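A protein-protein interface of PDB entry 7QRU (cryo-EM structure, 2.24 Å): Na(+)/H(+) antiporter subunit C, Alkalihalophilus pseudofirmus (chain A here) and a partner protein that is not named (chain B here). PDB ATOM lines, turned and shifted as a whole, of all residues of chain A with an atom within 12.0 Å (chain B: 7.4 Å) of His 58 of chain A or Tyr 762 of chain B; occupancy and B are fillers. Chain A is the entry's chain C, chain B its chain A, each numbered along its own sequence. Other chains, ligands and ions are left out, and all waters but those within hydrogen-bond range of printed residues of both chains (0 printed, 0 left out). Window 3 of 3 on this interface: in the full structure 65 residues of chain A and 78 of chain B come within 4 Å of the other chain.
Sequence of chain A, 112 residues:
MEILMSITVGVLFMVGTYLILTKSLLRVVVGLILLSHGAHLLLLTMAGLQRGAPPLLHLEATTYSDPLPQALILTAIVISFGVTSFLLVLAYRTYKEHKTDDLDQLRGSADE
The backbone carbonyl oxygen (O) of Tyr 762 of chain B lies within hydrogen-bond range of the backbone NH (N) of Leu 57 of chain A (2.9 Å).
N of Met 764 of chain B lies within hydrogen-bond range of O of Pro 55 of chain A (3.2 Å).
The side-chain hydroxyl (OG) of Ser 755 of chain B sits at hydrogen-bond distance from the backbone carbonyl oxygen (O) of Phe 751 of chain B (2.7 Å).
The backbone carbonyl oxygen (O) of Ser 755 of chain B sits at hydrogen-bond distance from the backbone NH (N) of Gly 760 of chain B (3.2 Å).
The side-chain amide oxygen (OD1) of Asn 763 of chain B lies close to the backbone NH (N) of Val 765 of chain B.
The side-chain amide oxygen (OD1) of Asn 763 of chain B is in hydrogen-bond range of the backbone NH (N) of Asn 766 of chain B, at 3.4 Å.
OH of Tyr 64 of chain A sits at hydrogen-bond distance from N of Glu 60 of chain A (3.4 Å).
The backbone NH (N) of Ala 61 of chain A sits at hydrogen-bond distance from the side-chain hydroxyl (OH) of Tyr 64 of chain A.
Among the printed residues, merely in contact across the chains: Pro 55 of chain A with Tyr 762 of chain B (3.9 Å), Pro 55 of chain A with Val 765 of chain B (3.8 Å), Leu 56 of chain A with Tyr 762 of chain B (3.5 Å), Leu 56 of chain A with Asn 763 of chain B (3.7 Å), Leu 57 of chain A with Ser 755 of chain B (3.8 Å), His 58 of chain A with Tyr 762 of chain B (3.7 Å), Tyr 64 of chain A with Met 764 of chain B (3.7 Å), Pro 67 of chain A with Met 764 of chain B (3.8 Å), Pro 67 of chain A with Val 765 of chain B (3.9 Å) and Gln 70 of chain A with Val 765 of chain B (3.7 Å).
Of the printed residues of chain B, Pro 55 of chain A touches Tyr 762, Met 764 and Val 765.
Of the printed residues of chain B, Leu 56 of chain A touches Tyr 762 and Asn 763.
Of the printed residues of chain B, His 58 of chain A touches Tyr 762 (3.7 Å).
Of the printed residues of chain B, Pro 67 of chain A touches Met 764 and Val 765.
Leu 68 of chain A touches none of the printed residues of chain B.
No residue of chain A comes within 4 Å of Lys 756 of chain B.
Tyr 762 of chain B touches four residues of chain A.
Of the printed residues of chain A, Asn 763 of chain B touches Leu 56.
Printed residues of chain A within 4 Å of Met 764 of chain B: Pro 55, Tyr 64 and Pro 67.
The nearest residue of chain B that does not touch His 58 of chain A is Asn 763 of chain B (5.9 Å).
The nearest printed residue of chain A that does not touch Tyr 762 of chain B is Glu 60 of chain A (6.3 Å).
Of the 12 printed residues of chain B, 5 touch a printed residue of chain A.
Hydrophobic or aromatic side chains of chain B within 4 Å of the printed part of chain A: Tyr 762, Met 764 and Val 765.
Among the printed residues, 12 pairs touch across the chains.
Among the printed residues, no Asp or Glu carboxylate lies within 4 Å of a Lys or Arg side-chain nitrogen of the other chain.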
ATOM      1  N   ALA A  53      -2.921 -10.680   7.351  1.00  0.00           N
ATOM      2  CA  ALA A  53      -1.993  -9.787   7.947  1.00  0.00           C
ATOM      3  C   ALA A  53      -2.608  -8.404   8.001  1.00  0.00           C
ATOM      4  O   ALA A  53      -3.439  -8.036   7.159  1.00  0.00           O
ATOM      5  CB  ALA A  53      -0.796  -9.823   7.061  1.00  0.00           C
ATOM      6  N   PRO A  54      -2.019  -7.502   8.776  1.00  0.00           N
ATOM      7  CA  PRO A  54      -2.376  -6.105   8.663  1.00  0.00           C
ATOM      8  C   PRO A  54      -2.135  -5.673   7.205  1.00  0.00           C
ATOM      9  O   PRO A  54      -1.290  -6.176   6.461  1.00  0.00           O
ATOM     10  CB  PRO A  54      -1.456  -5.393   9.663  1.00  0.00           C
ATOM     11  CG  PRO A  54      -0.836  -6.529  10.400  1.00  0.00           C
ATOM     12  CD  PRO A  54      -0.826  -7.751   9.526  1.00  0.00           C
ATOM     13  N   PRO A  55      -2.937  -4.756   6.677  1.00  0.00           N
ATOM     14  CA  PRO A  55      -2.906  -4.523   5.222  1.00  0.00           C
ATOM     15  C   PRO A  55      -1.751  -3.625   4.749  1.00  0.00           C
ATOM     16  O   PRO A  55      -1.968  -2.548   4.186  1.00  0.00           O
ATOM     17  CB  PRO A  55      -4.297  -3.935   4.983  1.00  0.00           C
ATOM     18  CG  PRO A  55      -4.724  -3.362   6.313  1.00  0.00           C
ATOM     19  CD  PRO A  55      -3.963  -4.037   7.430  1.00  0.00           C
ATOM     20  N   LEU A  56      -0.527  -4.207   4.809  1.00  0.00           N
ATOM     21  CA  LEU A  56       0.698  -3.515   4.462  1.00  0.00           C
ATOM     22  C   LEU A  56       1.442  -4.392   3.487  1.00  0.00           C
ATOM     23  O   LEU A  56       1.802  -5.471   3.909  1.00  0.00           O
ATOM     24  CB  LEU A  56       1.546  -3.261   5.680  1.00  0.00           C
ATOM     25  CG  LEU A  56       0.898  -2.368   6.723  1.00  0.00           C
ATOM     26  CD1 LEU A  56       1.737  -2.489   7.965  1.00  0.00           C
ATOM     27  CD2 LEU A  56       0.836  -0.901   6.302  1.00  0.00           C
ATOM     28  N   LEU A  57       1.485  -4.014   2.187  1.00  0.00           N
ATOM     29  CA  LEU A  57       1.856  -4.956   1.140  1.00  0.00           C
ATOM     30  C   LEU A  57       3.308  -5.377   1.224  1.00  0.00           C
ATOM     31  O   LEU A  57       3.683  -6.317   0.555  1.00  0.00           O
ATOM     32  CB  LEU A  57       1.576  -4.375  -0.242  1.00  0.00           C
ATOM     33  CG  LEU A  57       0.115  -4.415  -0.572  1.00  0.00           C
ATOM     34  CD1 LEU A  57      -0.203  -3.591  -1.840  1.00  0.00           C
ATOM     35  CD2 LEU A  57      -0.327  -5.828  -0.669  1.00  0.00           C
ATOM     36  N   HIS A  58       4.116  -4.616   1.905  1.00  0.00           N
ATOM     37  CA  HIS A  58       5.509  -4.979   1.988  1.00  0.00           C
ATOM     38  C   HIS A  58       5.709  -6.185   2.893  1.00  0.00           C
ATOM     39  O   HIS A  58       6.805  -6.708   2.903  1.00  0.00           O
ATOM     40  CB  HIS A  58       6.301  -3.774   2.477  1.00  0.00           C
ATOM     41  CG  HIS A  58       5.974  -3.320   3.842  1.00  0.00           C
ATOM     42  ND1 HIS A  58       6.224  -4.071   4.947  1.00  0.00           N
ATOM     43  CD2 HIS A  58       5.450  -2.140   4.241  1.00  0.00           C
ATOM     44  CE1 HIS A  58       5.882  -3.338   6.010  1.00  0.00           C
ATOM     45  NE2 HIS A  58       5.426  -2.106   5.612  1.00  0.00           N
ATOM     46  N   LEU A  59       4.652  -6.628   3.602  1.00  0.00           N
ATOM     47  CA  LEU A  59       4.729  -7.798   4.471  1.00  0.00           C
ATOM     48  C   LEU A  59       4.659  -9.034   3.609  1.00  0.00           C
ATOM     49  O   LEU A  59       4.957 -10.104   4.134  1.00  0.00           O
ATOM     50  CB  LEU A  59       3.624  -7.885   5.507  1.00  0.00           C
ATOM     51  CG  LEU A  59       3.571  -6.754   6.498  1.00  0.00           C
ATOM     52  CD1 LEU A  59       2.280  -6.821   7.317  1.00  0.00           C
ATOM     53  CD2 LEU A  59       4.737  -6.834   7.323  1.00  0.00           C
ATOM     54  N   GLU A  60       4.356  -8.870   2.326  1.00  0.00           N
ATOM     55  CA  GLU A  60       4.315  -9.993   1.397  1.00  0.00           C
ATOM     56  C   GLU A  60       3.602 -11.207   2.008  1.00  0.00           C
ATOM     57  O   GLU A  60       4.059 -12.340   1.854  1.00  0.00           O
ATOM     58  CB  GLU A  60       5.740 -10.324   0.995  1.00  0.00           C
ATOM     59  CG  GLU A  60       6.407  -9.204   0.228  1.00  0.00           C
ATOM     60  CD  GLU A  60       7.663  -9.560  -0.550  1.00  0.00           C
ATOM     61  OE1 GLU A  60       7.958 -10.772  -0.682  1.00  0.00           O
ATOM     62  OE2 GLU A  60       8.359  -8.619  -1.016  1.00  0.00           O
ATOM     63  N   ALA A  61       2.419 -10.977   2.619  1.00  0.00           N
ATOM     64  CA  ALA A  61       1.570 -12.024   3.185  1.00  0.00           C
ATOM     65  C   ALA A  61       0.707 -12.618   2.089  1.00  0.00           C
ATOM     66  O   ALA A  61       0.721 -12.115   0.961  1.00  0.00           O
ATOM     67  CB  ALA A  61       0.745 -11.423   4.227  1.00  0.00           C
ATOM     68  N   THR A  62       0.082 -13.763   2.388  1.00  0.00           N
ATOM     69  CA  THR A  62      -0.799 -14.441   1.435  1.00  0.00           C
ATOM     70  C   THR A  62      -2.187 -13.807   1.389  1.00  0.00           C
ATOM     71  O   THR A  62      -2.811 -13.708   0.324  1.00  0.00           O
ATOM     72  CB  THR A  62      -0.937 -15.936   1.762  1.00  0.00           C
ATOM     73  OG1 THR A  62      -1.342 -16.073   3.124  1.00  0.00           O
ATOM     74  CG2 THR A  62       0.379 -16.636   1.546  1.00  0.00           C
ATOM     75  N   THR A  63      -2.657 -13.436   2.565  1.00  0.00           N
ATOM     76  CA  THR A  63      -3.984 -12.924   2.783  1.00  0.00           C
ATOM     77  C   THR A  63      -3.795 -11.679   3.603  1.00  0.00           C
ATOM     78  O   THR A  63      -2.943 -11.653   4.436  1.00  0.00           O
ATOM     79  CB  THR A  63      -4.867 -14.012   3.424  1.00  0.00           C
ATOM     80  OG1 THR A  63      -5.293 -14.961   2.457  1.00  0.00           O
ATOM     81  CG2 THR A  63      -6.202 -13.489   3.822  1.00  0.00           C
ATOM     82  N   TYR A  64      -4.509 -10.632   3.308  1.00  0.00           N
ATOM     83  CA  TYR A  64      -4.450  -9.496   4.176  1.00  0.00           C
ATOM     84  C   TYR A  64      -5.809  -9.347   4.773  1.00  0.00           C
ATOM     85  O   TYR A  64      -6.723  -9.756   4.126  1.00  0.00           O
ATOM     86  CB  TYR A  64      -4.187  -8.240   3.385  1.00  0.00           C
ATOM     87  CG  TYR A  64      -2.832  -8.272   2.805  1.00  0.00           C
ATOM     88  CD1 TYR A  64      -1.787  -7.858   3.608  1.00  0.00           C
ATOM     89  CD2 TYR A  64      -2.607  -8.801   1.526  1.00  0.00           C
ATOM     90  CE1 TYR A  64      -0.492  -7.923   3.133  1.00  0.00           C
ATOM     91  CE2 TYR A  64      -1.315  -8.914   1.086  1.00  0.00           C
ATOM     92  CZ  TYR A  64      -0.257  -8.478   1.897  1.00  0.00           C
ATOM     93  OH  TYR A  64       1.065  -8.505   1.556  1.00  0.00           O
ATOM     94  N   SER A  65      -5.910  -8.782   5.981  1.00  0.00           N
ATOM     95  CA  SER A  65      -7.204  -8.379   6.499  1.00  0.00           C
ATOM     96  C   SER A  65      -7.783  -7.327   5.527  1.00  0.00           C
ATOM     97  O   SER A  65      -7.069  -6.567   4.950  1.00  0.00           O
ATOM     98  CB  SER A  65      -7.012  -7.810   7.822  1.00  0.00           C
ATOM     99  OG  SER A  65      -6.222  -6.619   7.593  1.00  0.00           O
ATOM    100  N   ASP A  66      -9.090  -7.217   5.389  1.00  0.00           N
ATOM    101  CA  ASP A  66      -9.699  -6.388   4.384  1.00  0.00           C
ATOM    102  C   ASP A  66      -9.420  -4.905   4.659  1.00  0.00           C
ATOM    103  O   ASP A  66      -9.731  -4.411   5.724  1.00  0.00           O
ATOM    104  CB  ASP A  66     -11.205  -6.642   4.421  1.00  0.00           C
ATOM    105  CG  ASP A  66     -11.997  -5.983   3.309  1.00  0.00           C
ATOM    106  OD1 ASP A  66     -11.402  -5.129   2.497  1.00  0.00           O
ATOM    107  OD2 ASP A  66     -13.176  -6.280   3.284  1.00  0.00           O
ATOM    108  N   PRO A  67      -8.773  -4.147   3.736  1.00  0.00           N
ATOM    109  CA  PRO A  67      -8.411  -2.777   4.023  1.00  0.00           C
ATOM    110  C   PRO A  67      -9.578  -1.831   3.790  1.00  0.00           C
ATOM    111  O   PRO A  67      -9.610  -0.782   4.432  1.00  0.00           O
ATOM    112  CB  PRO A  67      -7.352  -2.479   3.028  1.00  0.00           C
ATOM    113  CG  PRO A  67      -7.856  -3.276   1.832  1.00  0.00           C
ATOM    114  CD  PRO A  67      -8.251  -4.607   2.461  1.00  0.00           C
ATOM    115  N   LEU A  68     -10.601  -2.205   3.017  1.00  0.00           N
ATOM    116  CA  LEU A  68     -11.594  -1.179   2.766  1.00  0.00           C
ATOM    117  C   LEU A  68     -12.361  -0.782   4.013  1.00  0.00           C
ATOM    118  O   LEU A  68     -12.514   0.403   4.355  1.00  0.00           O
ATOM    119  CB  LEU A  68     -12.527  -1.615   1.668  1.00  0.00           C
ATOM    120  CG  LEU A  68     -13.636  -0.619   1.331  1.00  0.00           C
ATOM    121  CD1 LEU A  68     -13.151   0.749   1.042  1.00  0.00           C
ATOM    122  CD2 LEU A  68     -14.342  -1.183   0.127  1.00  0.00           C
ATOM    123  N   GLN A  70     -11.340  -0.790   7.103  1.00  0.00           N
ATOM    124  CA  GLN A  70     -10.440  -0.046   7.914  1.00  0.00           C
ATOM    125  C   GLN A  70     -10.456   1.371   7.430  1.00  0.00           C
ATOM    126  O   GLN A  70     -10.524   2.286   8.259  1.00  0.00           O
ATOM    127  CB  GLN A  70      -9.050  -0.684   7.860  1.00  0.00           C
ATOM    128  CG  GLN A  70      -9.007  -2.104   8.443  1.00  0.00           C
ATOM    129  CD  GLN A  70      -7.611  -2.619   8.720  1.00  0.00           C
ATOM    130  OE1 GLN A  70      -6.732  -1.795   8.947  1.00  0.00           O
ATOM    131  NE2 GLN A  70      -7.392  -3.947   8.831  1.00  0.00           N
ATOM    132  N   PHE B 751      -7.650  -3.297  -4.553  1.00  0.00           N
ATOM    133  CA  PHE B 751      -6.712  -2.545  -3.798  1.00  0.00           C
ATOM    134  C   PHE B 751      -5.536  -3.426  -3.359  1.00  0.00           C
ATOM    135  O   PHE B 751      -4.390  -2.989  -3.262  1.00  0.00           O
ATOM    136  CB  PHE B 751      -7.429  -1.984  -2.555  1.00  0.00           C
ATOM    137  CG  PHE B 751      -8.699  -1.246  -2.826  1.00  0.00           C
ATOM    138  CD1 PHE B 751      -8.823  -0.366  -3.898  1.00  0.00           C
ATOM    139  CD2 PHE B 751      -9.770  -1.344  -1.946  1.00  0.00           C
ATOM    140  CE1 PHE B 751     -10.000   0.331  -4.129  1.00  0.00           C
ATOM    141  CE2 PHE B 751     -10.964  -0.671  -2.199  1.00  0.00           C
ATOM    142  CZ  PHE B 751     -11.086   0.142  -3.305  1.00  0.00           C
ATOM    143  N   SER B 755      -2.631  -1.488  -5.180  1.00  0.00           N
ATOM    144  CA  SER B 755      -2.149  -0.364  -4.384  1.00  0.00           C
ATOM    145  C   SER B 755      -0.717  -0.031  -4.752  1.00  0.00           C
ATOM    146  O   SER B 755      -0.364   1.134  -4.664  1.00  0.00           O
ATOM    147  CB  SER B 755      -2.200  -0.506  -2.877  1.00  0.00           C
ATOM    148  OG  SER B 755      -3.539  -0.581  -2.529  1.00  0.00           O
ATOM    149  N   LYS B 756       0.182  -0.999  -4.949  1.00  0.00           N
ATOM    150  CA  LYS B 756       1.545  -0.517  -5.119  1.00  0.00           C
ATOM    151  C   LYS B 756       1.759  -0.183  -6.601  1.00  0.00           C
ATOM    152  O   LYS B 756       2.235   0.901  -6.869  1.00  0.00           O
ATOM    153  CB  LYS B 756       2.625  -1.470  -4.603  1.00  0.00           C
ATOM    154  CG  LYS B 756       4.060  -0.971  -4.795  1.00  0.00           C
ATOM    155  CD  LYS B 756       4.292   0.300  -3.973  1.00  0.00           C
ATOM    156  CE  LYS B 756       5.738   0.656  -3.679  1.00  0.00           C
ATOM    157  NZ  LYS B 756       6.517   0.480  -4.921  1.00  0.00           N
ATOM    158  N   ALA B 759      -0.815   2.846  -7.547  1.00  0.00           N
ATOM    159  CA  ALA B 759      -0.976   4.039  -6.720  1.00  0.00           C
ATOM    160  C   ALA B 759       0.248   4.267  -5.898  1.00  0.00           C
ATOM    161  O   ALA B 759       0.269   5.188  -5.119  1.00  0.00           O
ATOM    162  CB  ALA B 759      -2.217   3.930  -5.879  1.00  0.00           C
ATOM    163  N   GLY B 760       1.278   3.470  -6.125  1.00  0.00           N
ATOM    164  CA  GLY B 760       2.525   3.749  -5.495  1.00  0.00           C
ATOM    165  C   GLY B 760       2.626   3.642  -3.970  1.00  0.00           C
ATOM    166  O   GLY B 760       3.635   4.064  -3.460  1.00  0.00           O
ATOM    167  N   GLY B 761       1.748   2.971  -3.222  1.00  0.00           N
ATOM    168  CA  GLY B 761       2.035   2.840  -1.805  1.00  0.00           C
ATOM    169  C   GLY B 761       1.896   1.410  -1.344  1.00  0.00           C
ATOM    170  O   GLY B 761       1.189   0.670  -1.958  1.00  0.00           O
ATOM    171  N   TYR B 762       2.491   1.070  -0.231  1.00  0.00           N
ATOM    172  CA  TYR B 762       2.305  -0.230   0.343  1.00  0.00           C
ATOM    173  C   TYR B 762       1.261  -0.254   1.454  1.00  0.00           C
ATOM    174  O   TYR B 762       0.743  -1.297   1.694  1.00  0.00           O
ATOM    175  CB  TYR B 762       3.543  -0.628   1.076  1.00  0.00           C
ATOM    176  CG  TYR B 762       4.635  -1.057   0.173  1.00  0.00           C
ATOM    177  CD1 TYR B 762       4.402  -2.044  -0.760  1.00  0.00           C
ATOM    178  CD2 TYR B 762       5.903  -0.547   0.332  1.00  0.00           C
ATOM    179  CE1 TYR B 762       5.441  -2.506  -1.539  1.00  0.00           C
ATOM    180  CE2 TYR B 762       6.948  -1.034  -0.424  1.00  0.00           C
ATOM    181  CZ  TYR B 762       6.721  -2.039  -1.332  1.00  0.00           C
ATOM    182  OH  TYR B 762       7.732  -2.441  -2.167  1.00  0.00           O
ATOM    183  N   ASN B 763       0.900   0.862   2.055  1.00  0.00           N
ATOM    184  CA  ASN B 763      -0.123   0.908   3.084  1.00  0.00           C
ATOM    185  C   ASN B 763      -1.520   1.019   2.405  1.00  0.00           C
ATOM    186  O   ASN B 763      -1.924   2.089   2.018  1.00  0.00           O
ATOM    187  CB  ASN B 763       0.242   2.074   3.975  1.00  0.00           C
ATOM    188  CG  ASN B 763      -0.765   2.256   5.079  1.00  0.00           C
ATOM    189  OD1 ASN B 763      -1.789   1.560   5.092  1.00  0.00           O
ATOM    190  ND2 ASN B 763      -0.523   3.242   5.940  1.00  0.00           N
ATOM    191  N   MET B 764      -2.206  -0.099   2.171  1.00  0.00           N
ATOM    192  CA  MET B 764      -3.489  -0.128   1.531  1.00  0.00           C
ATOM    193  C   MET B 764      -4.519   0.761   2.201  1.00  0.00           C
ATOM    194  O   MET B 764      -5.186   1.451   1.473  1.00  0.00           O
ATOM    195  CB  MET B 764      -4.053  -1.501   1.486  1.00  0.00           C
ATOM    196  CG  MET B 764      -3.232  -2.316   0.629  1.00  0.00           C
ATOM    197  SD  MET B 764      -3.975  -3.914   0.290  1.00  0.00           S
ATOM    198  CE  MET B 764      -3.640  -4.835   1.770  1.00  0.00           C
ATOM    199  N   VAL B 765      -4.487   0.961   3.486  1.00  0.00           N
ATOM    200  CA  VAL B 765      -5.496   1.814   4.023  1.00  0.00           C
ATOM    201  C   VAL B 765      -5.188   3.250   3.592  1.00  0.00           C
ATOM    202  O   VAL B 765      -6.062   3.923   3.113  1.00  0.00           O
ATOM    203  CB  VAL B 765      -5.595   1.586   5.546  1.00  0.00           C
ATOM    204  CG1 VAL B 765      -6.499   2.536   6.267  1.00  0.00           C
ATOM    205  CG2 VAL B 765      -6.062   0.180   5.800  1.00  0.00           C
ATOM    206  N   ASN B 766      -3.964   3.744   3.750  1.00  0.00           N
ATOM    207  CA  ASN B 766      -3.652   5.120   3.354  1.00  0.00           C
ATOM    208  C   ASN B 766      -3.897   5.325   1.867  1.00  0.00           C
ATOM    209  O   ASN B 766      -4.355   6.377   1.494  1.00  0.00           O
ATOM    210  CB  ASN B 766      -2.221   5.536   3.668  1.00  0.00           C
ATOM    211  CG  ASN B 766      -2.002   7.046   3.633  1.00  0.00           C
ATOM    212  OD1 ASN B 766      -2.481   7.748   4.526  1.00  0.00           O
ATOM    213  ND2 ASN B 766      -1.296   7.531   2.605  1.00  0.00           N
ATOM    214  N   VAL B 767      -3.616   4.326   1.035  1.00  0.00           N
ATOM    215  CA  VAL B 767      -3.785   4.471  -0.367  1.00  0.00           C
ATOM    216  C   VAL B 767      -5.275   4.616  -0.676  1.00  0.00           C
ATOM    217  O   VAL B 767      -5.663   5.271  -1.608  1.00  0.00           O
ATOM    218  CB  VAL B 767      -3.070   3.332  -1.080  1.00  0.00           C
ATOM    219  CG1 VAL B 767      -3.407   3.299  -2.529  1.00  0.00           C
ATOM    220  CG2 VAL B 767      -1.533   3.485  -0.882  1.00  0.00           C
